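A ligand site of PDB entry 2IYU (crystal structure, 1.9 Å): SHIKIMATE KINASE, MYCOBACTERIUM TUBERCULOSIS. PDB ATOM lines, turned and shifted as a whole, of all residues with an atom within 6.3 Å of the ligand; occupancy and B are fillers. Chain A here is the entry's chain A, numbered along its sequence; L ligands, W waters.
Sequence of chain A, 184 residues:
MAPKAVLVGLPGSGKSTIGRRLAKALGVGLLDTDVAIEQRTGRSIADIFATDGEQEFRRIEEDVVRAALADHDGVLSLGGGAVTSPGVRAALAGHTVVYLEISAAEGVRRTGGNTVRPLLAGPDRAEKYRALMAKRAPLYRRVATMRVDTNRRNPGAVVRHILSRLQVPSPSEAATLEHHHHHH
An oxygen (O5) of the ligand sits at hydrogen-bond distance from the backbone NH (N) of Thr 17 (2.8 Å). An oxygen (O5) of the ligand sits at hydrogen-bond distance from the side-chain hydroxyl (OG1) of Thr 17. The backbone NH (N) of Lys 15 is in hydrogen-bond range of an oxygen (O3) of the ligand, at 2.7 Å. The side-chain amino group (NZ) of Lys 15 is in salt-bridge range of an oxygen (O3) of the ligand, 3.1 Å away. The backbone carbonyl oxygen (O) of Arg 153 is in hydrogen-bond range of a nitrogen (N3) of the ligand (2.8 Å). An oxygen (O1) of the ligand lies within hydrogen-bond range of the backbone NH (N) of Ser 16 (3.0 Å). The side-chain hydroxyl (OG) of Ser 16 is in hydrogen-bond range of an oxygen (O1) of the ligand (2.9 Å). An oxygen (O3) of the ligand sits at hydrogen-bond distance from the backbone NH (N) of Gly 14 (3.0 Å). The backbone NH (N) of Gly 12 is in hydrogen-bond range of an oxygen (O2) of the ligand (3.3 Å).
NZ of Lys 15 lies within hydrogen-bond range of O of Leu 10 (3.0 Å). O of Gly 9 is in hydrogen-bond range of NZ of Lys 15, 2.7 Å away. The backbone carbonyl oxygen (O) of Gly 12 lies close to the guanidinium group (NH1) of Arg 110, at 3.1 Å. The guanidinium group (NH2) of Arg 110 lies within hydrogen-bond range of the backbone carbonyl oxygen (O) of Thr 150, at 2.8 Å. OE2 of Glu 106 lies within salt-bridge range of NH2 of Arg 110 (3.2 Å). The side-chain hydroxyl (OG) of Ser 13 is in hydrogen-bond range of the backbone carbonyl oxygen (O) of Leu 10 (2.6 Å).
Merely in contact with the ligand: Leu 10 (3.7 Å), Pro 11 (3.7 Å), Ser 13 (3.6 Å), Arg 110 (3.4 Å), Thr 150 (3.9 Å), Asn 154 (3.9 Å) and Pro 155 (3.7 Å). Hydrophobic or aromatic side chains within 4 Å of the ligand: Pro 155. Within 4 Å of the ligand: Leu 10, Pro 11, Gly 12, Ser 13, Gly 14, Lys 15, Ser 16, Thr 17, Arg 110, Thr 150, Arg 153, Asn 154 and Pro 155. The nearest printed residue that does not touch the ligand is Val 158 (4.1 Å).
Water W4 lies within hydrogen-bond range of N4 of the ligand and O of Arg 153. Water W2 lies within hydrogen-bond range of N2 of the ligand (2.8 Å) and O of Ser 13 (2.9 Å). Water W1 bridges NH2 of Arg 109 and N5 of the ligand.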
ATOM      1  N   GLY A   9      -2.803  -0.067  22.642  1.00  0.00           N
ATOM      2  CA  GLY A   9      -3.776  -0.078  21.565  1.00  0.00           C
ATOM      3  C   GLY A   9      -5.196  -0.079  22.125  1.00  0.00           C
ATOM      4  O   GLY A   9      -5.427  -0.264  23.335  1.00  0.00           O
ATOM      5  N   LEU A  10      -6.161   0.120  21.249  1.00  0.00           N
ATOM      6  CA  LEU A  10      -7.553   0.104  21.644  1.00  0.00           C
ATOM      7  C   LEU A  10      -8.048  -1.262  22.121  1.00  0.00           C
ATOM      8  O   LEU A  10      -7.392  -2.259  21.928  1.00  0.00           O
ATOM      9  CB  LEU A  10      -8.441   0.512  20.460  1.00  0.00           C
ATOM     10  CG  LEU A  10      -8.628   1.978  20.109  1.00  0.00           C
ATOM     11  CD1 LEU A  10      -8.932   2.812  21.311  1.00  0.00           C
ATOM     12  CD2 LEU A  10      -7.418   2.501  19.394  1.00  0.00           C
ATOM     13  N   PRO A  11      -9.281  -1.325  22.678  1.00  0.00           N
ATOM     14  CA  PRO A  11      -9.839  -2.691  22.809  1.00  0.00           C
ATOM     15  C   PRO A  11      -9.994  -3.435  21.472  1.00  0.00           C
ATOM     16  O   PRO A  11     -10.444  -2.890  20.481  1.00  0.00           O
ATOM     17  CB  PRO A  11     -11.217  -2.444  23.495  1.00  0.00           C
ATOM     18  CG  PRO A  11     -11.146  -1.034  24.092  1.00  0.00           C
ATOM     19  CD  PRO A  11     -10.173  -0.279  23.215  1.00  0.00           C
ATOM     20  N   GLY A  12      -9.649  -4.719  21.454  1.00  0.00           N
ATOM     21  CA  GLY A  12      -9.683  -5.497  20.232  1.00  0.00           C
ATOM     22  C   GLY A  12      -8.384  -5.531  19.482  1.00  0.00           C
ATOM     23  O   GLY A  12      -8.219  -6.370  18.602  1.00  0.00           O
ATOM     24  N   SER A  13      -7.434  -4.630  19.814  1.00  0.00           N
ATOM     25  CA  SER A  13      -6.236  -4.526  19.028  1.00  0.00           C
ATOM     26  C   SER A  13      -5.355  -5.731  19.212  1.00  0.00           C
ATOM     27  O   SER A  13      -4.616  -6.065  18.315  1.00  0.00           O
ATOM     28  CB  SER A  13      -5.446  -3.246  19.336  1.00  0.00           C
ATOM     29  OG  SER A  13      -5.252  -3.108  20.729  1.00  0.00           O
ATOM     30  N   GLY A  14      -5.480  -6.400  20.371  1.00  0.00           N
ATOM     31  CA  GLY A  14      -4.838  -7.650  20.618  1.00  0.00           C
ATOM     32  C   GLY A  14      -3.793  -7.639  21.701  1.00  0.00           C
ATOM     33  O   GLY A  14      -2.919  -8.457  21.633  1.00  0.00           O
ATOM     34  N   LYS A  15      -3.903  -6.740  22.679  1.00  0.00           N
ATOM     35  CA  LYS A  15      -2.849  -6.563  23.749  1.00  0.00           C
ATOM     36  C   LYS A  15      -2.708  -7.859  24.516  1.00  0.00           C
ATOM     37  O   LYS A  15      -1.587  -8.292  24.808  1.00  0.00           O
ATOM     38  CB  LYS A  15      -3.166  -5.407  24.711  1.00  0.00           C
ATOM     39  CG  LYS A  15      -3.115  -3.980  24.048  1.00  0.00           C
ATOM     40  CD  LYS A  15      -3.367  -2.823  25.001  1.00  0.00           C
ATOM     41  CE  LYS A  15      -4.802  -2.754  25.513  1.00  0.00           C
ATOM     42  NZ  LYS A  15      -5.815  -2.747  24.397  1.00  0.00           N
ATOM     43  N   SER A  16      -3.833  -8.445  24.869  1.00  0.00           N
ATOM     44  CA  SER A  16      -3.856  -9.747  25.556  1.00  0.00           C
ATOM     45  C   SER A  16      -3.352 -10.839  24.673  1.00  0.00           C
ATOM     46  O   SER A  16      -2.419 -11.561  25.044  1.00  0.00           O
ATOM     47  CB  SER A  16      -5.255 -10.055  26.122  1.00  0.00           C
ATOM     48  OG  SER A  16      -5.654  -9.114  27.093  1.00  0.00           O
ATOM     49  N   THR A  17      -3.901 -10.959  23.458  1.00  0.00           N
ATOM     50  CA  THR A  17      -3.521 -12.010  22.572  1.00  0.00           C
ATOM     51  C   THR A  17      -2.068 -11.936  22.120  1.00  0.00           C
ATOM     52  O   THR A  17      -1.365 -12.917  22.085  1.00  0.00           O
ATOM     53  CB  THR A  17      -4.428 -11.984  21.312  1.00  0.00           C
ATOM     54  OG1 THR A  17      -5.805 -12.045  21.722  1.00  0.00           O
ATOM     55  CG2 THR A  17      -4.085 -13.090  20.408  1.00  0.00           C
ATOM     56  N   ILE A  18      -1.644 -10.762  21.687  1.00  0.00           N
ATOM     57  CA  ILE A  18      -0.293 -10.616  21.162  1.00  0.00           C
ATOM     58  C   ILE A  18       0.737 -10.604  22.293  1.00  0.00           C
ATOM     59  O   ILE A  18       1.854 -11.088  22.072  1.00  0.00           O
ATOM     60  CB  ILE A  18      -0.164  -9.379  20.253  1.00  0.00           C
ATOM     61  CG1 ILE A  18      -1.219  -9.415  19.134  1.00  0.00           C
ATOM     62  CG2 ILE A  18       1.284  -9.213  19.685  1.00  0.00           C
ATOM     63  CD1 ILE A  18      -1.087 -10.514  18.167  1.00  0.00           C
ATOM     64  N   ARG A  20       0.557 -12.312  25.076  1.00  0.00           N
ATOM     65  CA  ARG A  20       0.815 -13.740  25.297  1.00  0.00           C
ATOM     66  C   ARG A  20       1.758 -14.392  24.281  1.00  0.00           C
ATOM     67  O   ARG A  20       2.814 -14.990  24.637  1.00  0.00           O
ATOM     68  CB  ARG A  20      -0.551 -14.455  25.294  1.00  0.00           C
ATOM     69  CG  ARG A  20      -0.617 -15.781  26.054  1.00  0.00           C
ATOM     70  CD  ARG A  20      -2.056 -16.141  26.467  1.00  0.00           C
ATOM     71  NE  ARG A  20      -3.086 -15.351  25.763  1.00  0.00           N
ATOM     72  CZ  ARG A  20      -4.372 -15.673  25.632  1.00  0.00           C
ATOM     73  NH1 ARG A  20      -4.865 -16.795  26.162  1.00  0.00           N
ATOM     74  NH2 ARG A  20      -5.178 -14.862  24.946  1.00  0.00           N
ATOM     75  N   SER A  77       1.973  -5.119  28.925  1.00  0.00           N
ATOM     76  CA  SER A  77       0.701  -4.738  28.291  1.00  0.00           C
ATOM     77  C   SER A  77       0.077  -3.600  29.091  1.00  0.00           C
ATOM     78  O   SER A  77      -0.255  -3.778  30.293  1.00  0.00           O
ATOM     79  CB  SER A  77      -0.183  -5.985  28.300  1.00  0.00           C
ATOM     80  OG  SER A  77      -1.361  -5.698  27.623  1.00  0.00           O
ATOM     81  N   LEU A 100      -0.428  -1.378  18.585  1.00  0.00           N
ATOM     82  CA  LEU A 100      -1.285  -2.323  17.866  1.00  0.00           C
ATOM     83  C   LEU A 100      -2.516  -1.496  17.314  1.00  0.00           C
ATOM     84  O   LEU A 100      -3.504  -1.185  18.029  1.00  0.00           O
ATOM     85  CB  LEU A 100      -1.787  -3.439  18.811  1.00  0.00           C
ATOM     86  CG  LEU A 100      -0.728  -4.355  19.441  1.00  0.00           C
ATOM     87  CD1 LEU A 100      -1.310  -5.388  20.454  1.00  0.00           C
ATOM     88  CD2 LEU A 100       0.157  -4.964  18.413  1.00  0.00           C
ATOM     89  N   GLU A 106     -13.127  -3.157  12.727  1.00  0.00           N
ATOM     90  CA  GLU A 106     -12.513  -4.362  13.247  1.00  0.00           C
ATOM     91  C   GLU A 106     -12.548  -4.354  14.762  1.00  0.00           C
ATOM     92  O   GLU A 106     -12.807  -5.399  15.425  1.00  0.00           O
ATOM     93  CB  GLU A 106     -11.070  -4.467  12.740  1.00  0.00           C
ATOM     94  CG  GLU A 106     -10.462  -5.868  12.876  1.00  0.00           C
ATOM     95  CD  GLU A 106     -10.556  -6.690  11.608  1.00  0.00           C
ATOM     96  OE1 GLU A 106     -11.684  -6.819  11.072  1.00  0.00           O
ATOM     97  OE2 GLU A 106      -9.510  -7.234  11.165  1.00  0.00           O
ATOM     98  N   ARG A 109     -15.965  -5.409  15.897  1.00  0.00           N
ATOM     99  CA  ARG A 109     -16.101  -6.844  15.619  1.00  0.00           C
ATOM    100  C   ARG A 109     -15.403  -7.734  16.657  1.00  0.00           C
ATOM    101  O   ARG A 109     -15.960  -8.713  17.170  1.00  0.00           O
ATOM    102  CB  ARG A 109     -15.608  -7.136  14.184  1.00  0.00           C
ATOM    103  CG  ARG A 109     -15.622  -8.622  13.810  1.00  0.00           C
ATOM    104  CD  ARG A 109     -14.885  -8.892  12.504  1.00  0.00           C
ATOM    105  NE  ARG A 109     -13.974 -10.018  12.632  1.00  0.00           N
ATOM    106  CZ  ARG A 109     -12.673  -9.942  12.967  1.00  0.00           C
ATOM    107  NH1 ARG A 109     -12.091  -8.773  13.229  1.00  0.00           N
ATOM    108  NH2 ARG A 109     -11.956 -11.058  13.046  1.00  0.00           N
ATOM    109  N   ARG A 110     -14.171  -7.389  17.005  1.00  0.00           N
ATOM    110  CA  ARG A 110     -13.378  -8.241  17.905  1.00  0.00           C
ATOM    111  C   ARG A 110     -13.876  -8.181  19.368  1.00  0.00           C
ATOM    112  O   ARG A 110     -13.626  -9.080  20.158  1.00  0.00           O
ATOM    113  CB  ARG A 110     -11.906  -7.833  17.805  1.00  0.00           C
ATOM    114  CG  ARG A 110     -11.295  -8.135  16.464  1.00  0.00           C
ATOM    115  CD  ARG A 110      -9.785  -7.862  16.538  1.00  0.00           C
ATOM    116  NE  ARG A 110      -9.205  -7.854  15.226  1.00  0.00           N
ATOM    117  CZ  ARG A 110      -7.982  -7.457  14.909  1.00  0.00           C
ATOM    118  NH1 ARG A 110      -7.136  -7.013  15.822  1.00  0.00           N
ATOM    119  NH2 ARG A 110      -7.588  -7.501  13.654  1.00  0.00           N
ATOM    120  N   THR A 111     -14.558  -7.090  19.729  1.00  0.00           N
ATOM    121  CA  THR A 111     -15.056  -6.922  21.065  1.00  0.00           C
ATOM    122  C   THR A 111     -16.583  -7.202  21.045  1.00  0.00           C
ATOM    123  O   THR A 111     -17.249  -6.965  22.041  1.00  0.00           O
ATOM    124  CB  THR A 111     -14.789  -5.468  21.601  1.00  0.00           C
ATOM    125  OG1 THR A 111     -15.446  -4.525  20.783  1.00  0.00           O
ATOM    126  CG2 THR A 111     -13.259  -5.102  21.618  1.00  0.00           C
ATOM    127  N   THR A 150      -2.922  -4.236  12.642  1.00  0.00           N
ATOM    128  CA  THR A 150      -3.387  -5.581  12.952  1.00  0.00           C
ATOM    129  C   THR A 150      -4.660  -5.924  12.182  1.00  0.00           C
ATOM    130  O   THR A 150      -5.166  -6.991  12.373  1.00  0.00           O
ATOM    131  CB  THR A 150      -3.631  -5.818  14.478  1.00  0.00           C
ATOM    132  OG1 THR A 150      -4.852  -5.219  14.919  1.00  0.00           O
ATOM    133  CG2 THR A 150      -2.479  -5.204  15.296  1.00  0.00           C
ATOM    134  N   ASN A 151      -5.157  -4.969  11.384  1.00  0.00           N
ATOM    135  CA  ASN A 151      -6.353  -5.114  10.514  1.00  0.00           C
ATOM    136  C   ASN A 151      -6.071  -6.142   9.438  1.00  0.00           C
ATOM    137  O   ASN A 151      -5.164  -5.964   8.618  1.00  0.00           O
ATOM    138  CB  ASN A 151      -6.664  -3.801   9.832  1.00  0.00           C
ATOM    139  CG  ASN A 151      -7.231  -2.774  10.777  1.00  0.00           C
ATOM    140  OD1 ASN A 151      -8.313  -2.972  11.341  1.00  0.00           O
ATOM    141  ND2 ASN A 151      -6.520  -1.664  10.951  1.00  0.00           N
ATOM    142  N   ARG A 152      -6.841  -7.241   9.463  1.00  0.00           N
ATOM    143  CA  ARG A 152      -6.681  -8.381   8.537  1.00  0.00           C
ATOM    144  C   ARG A 152      -5.317  -9.012   8.596  1.00  0.00           C
ATOM    145  O   ARG A 152      -4.807  -9.440   7.581  1.00  0.00           O
ATOM    146  CB  ARG A 152      -7.082  -8.015   7.085  1.00  0.00           C
ATOM    147  CG  ARG A 152      -8.591  -7.856   6.909  1.00  0.00           C
ATOM    148  CD  ARG A 152      -8.962  -6.431   6.714  1.00  0.00           C
ATOM    149  NE  ARG A 152      -8.590  -5.973   5.373  1.00  0.00           N
ATOM    150  CZ  ARG A 152      -8.851  -4.749   4.895  1.00  0.00           C
ATOM    151  NH1 ARG A 152      -9.503  -3.846   5.628  1.00  0.00           N
ATOM    152  NH2 ARG A 152      -8.477  -4.433   3.671  1.00  0.00           N
ATOM    153  N   ARG A 153      -4.726  -9.053   9.795  1.00  0.00           N
ATOM    154  CA  ARG A 153      -3.567  -9.910  10.062  1.00  0.00           C
ATOM    155  C   ARG A 153      -3.853 -10.909  11.168  1.00  0.00           C
ATOM    156  O   ARG A 153      -4.558 -10.603  12.124  1.00  0.00           O
ATOM    157  CB  ARG A 153      -2.347  -9.082  10.355  1.00  0.00           C
ATOM    158  CG  ARG A 153      -2.045  -8.172   9.220  1.00  0.00           C
ATOM    159  CD  ARG A 153      -1.069  -7.166   9.617  1.00  0.00           C
ATOM    160  NE  ARG A 153       0.277  -7.602   9.367  1.00  0.00           N
ATOM    161  CZ  ARG A 153       1.329  -6.798   9.383  1.00  0.00           C
ATOM    162  NH1 ARG A 153       1.172  -5.492   9.646  1.00  0.00           N
ATOM    163  NH2 ARG A 153       2.537  -7.286   9.137  1.00  0.00           N
ATOM    164  N   ASN A 154      -3.352 -12.115  10.984  1.00  0.00           N
ATOM    165  CA  ASN A 154      -3.418 -13.177  11.978  1.00  0.00           C
ATOM    166  C   ASN A 154      -2.499 -12.745  13.172  1.00  0.00           C
ATOM    167  O   ASN A 154      -1.510 -12.039  12.933  1.00  0.00           O
ATOM    168  CB  ASN A 154      -2.894 -14.475  11.320  1.00  0.00           C
ATOM    169  CG  ASN A 154      -3.086 -15.722  12.194  1.00  0.00           C
ATOM    170  OD1 ASN A 154      -2.115 -16.331  12.694  1.00  0.00           O
ATOM    171  ND2 ASN A 154      -4.342 -16.110  12.376  1.00  0.00           N
ATOM    172  N   PRO A 155      -2.835 -13.146  14.397  1.00  0.00           N
ATOM    173  CA  PRO A 155      -1.906 -12.978  15.531  1.00  0.00           C
ATOM    174  C   PRO A 155      -0.476 -13.463  15.278  1.00  0.00           C
ATOM    175  O   PRO A 155       0.476 -12.789  15.650  1.00  0.00           O
ATOM    176  CB  PRO A 155      -2.594 -13.757  16.677  1.00  0.00           C
ATOM    177  CG  PRO A 155      -4.003 -13.725  16.330  1.00  0.00           C
ATOM    178  CD  PRO A 155      -4.140 -13.701  14.834  1.00  0.00           C
ATOM    179  N   VAL A 158       1.171 -10.798  13.094  1.00  0.00           N
ATOM    180  CA  VAL A 158       1.476  -9.584  13.902  1.00  0.00           C
ATOM    181  C   VAL A 158       2.732  -9.861  14.738  1.00  0.00           C
ATOM    182  O   VAL A 158       3.681  -9.045  14.821  1.00  0.00           O
ATOM    183  CB  VAL A 158       0.287  -9.193  14.774  1.00  0.00           C
ATOM    184  CG1 VAL A 158       0.672  -8.096  15.793  1.00  0.00           C
ATOM    185  CG2 VAL A 158      -0.871  -8.720  13.910  1.00  0.00           C
HETATM  186  P1  LIG L   1      -7.160  -6.435  24.002  1.00  0.00           P
HETATM  187  O1  LIG L   1      -6.452  -7.091  25.168  1.00  0.00           O
HETATM  188  O2  LIG L   1      -8.516  -5.816  24.338  1.00  0.00           O
HETATM  189  O3  LIG L   1      -6.291  -5.515  23.173  1.00  0.00           O
HETATM  190  P2  LIG L   1      -7.565  -9.131  22.898  1.00  0.00           P
HETATM  191  O4  LIG L   1      -8.268  -9.385  24.179  1.00  0.00           O
HETATM  192  O5  LIG L   1      -6.172  -9.665  22.516  1.00  0.00           O
HETATM  193  O6  LIG L   1      -7.472  -7.512  22.881  1.00  0.00           O
HETATM  194  O7  LIG L   1      -8.392  -9.462  21.580  1.00  0.00           O
HETATM  195  C1  LIG L   1      -9.810  -9.305  21.551  1.00  0.00           C
HETATM  196  C2  LIG L   1     -10.355 -10.440  20.717  1.00  0.00           C
HETATM  197  O8  LIG L   1     -10.029 -10.153  19.371  1.00  0.00           O
HETATM  198  C3  LIG L   1      -9.840 -11.858  20.987  1.00  0.00           C
HETATM  199  O9  LIG L   1     -10.940 -12.784  20.912  1.00  0.00           O
HETATM  200  C4  LIG L   1      -8.872 -12.133  19.854  1.00  0.00           C
HETATM  201  O10 LIG L   1      -8.857 -13.462  19.359  1.00  0.00           O
HETATM  202  C5  LIG L   1      -9.291 -11.163  18.762  1.00  0.00           C
HETATM  203  N1  LIG L   1      -8.057 -10.681  18.101  1.00  0.00           N
HETATM  204  C6  LIG L   1      -6.990 -10.074  18.677  1.00  0.00           C
HETATM  205  N2  LIG L   1      -6.010  -9.847  17.759  1.00  0.00           N
HETATM  206  C7  LIG L   1      -6.442 -10.361  16.568  1.00  0.00           C
HETATM  207  C8  LIG L   1      -5.940 -10.471  15.159  1.00  0.00           C
HETATM  208  N3  LIG L   1      -4.695  -9.988  14.844  1.00  0.00           N
HETATM  209  N4  LIG L   1      -6.765 -11.090  14.223  1.00  0.00           N
HETATM  210  C9  LIG L   1      -7.996 -11.546  14.561  1.00  0.00           C
HETATM  211  N5  LIG L   1      -8.507 -11.437  15.796  1.00  0.00           N
HETATM  212  C10 LIG L   1      -7.796 -10.901  16.821  1.00  0.00           C
HETATM  213  O   HOH W   1     -11.591 -12.059  15.680  1.00  0.00           O
HETATM  214  O   HOH W   2      -3.690  -8.442  17.013  1.00  0.00           O
HETATM  215  O   HOH W   3     -11.094  -7.107  24.946  1.00  0.00           O
HETATM  216  O   HOH W   4      -7.254 -12.104  11.815  1.00  0.00           O
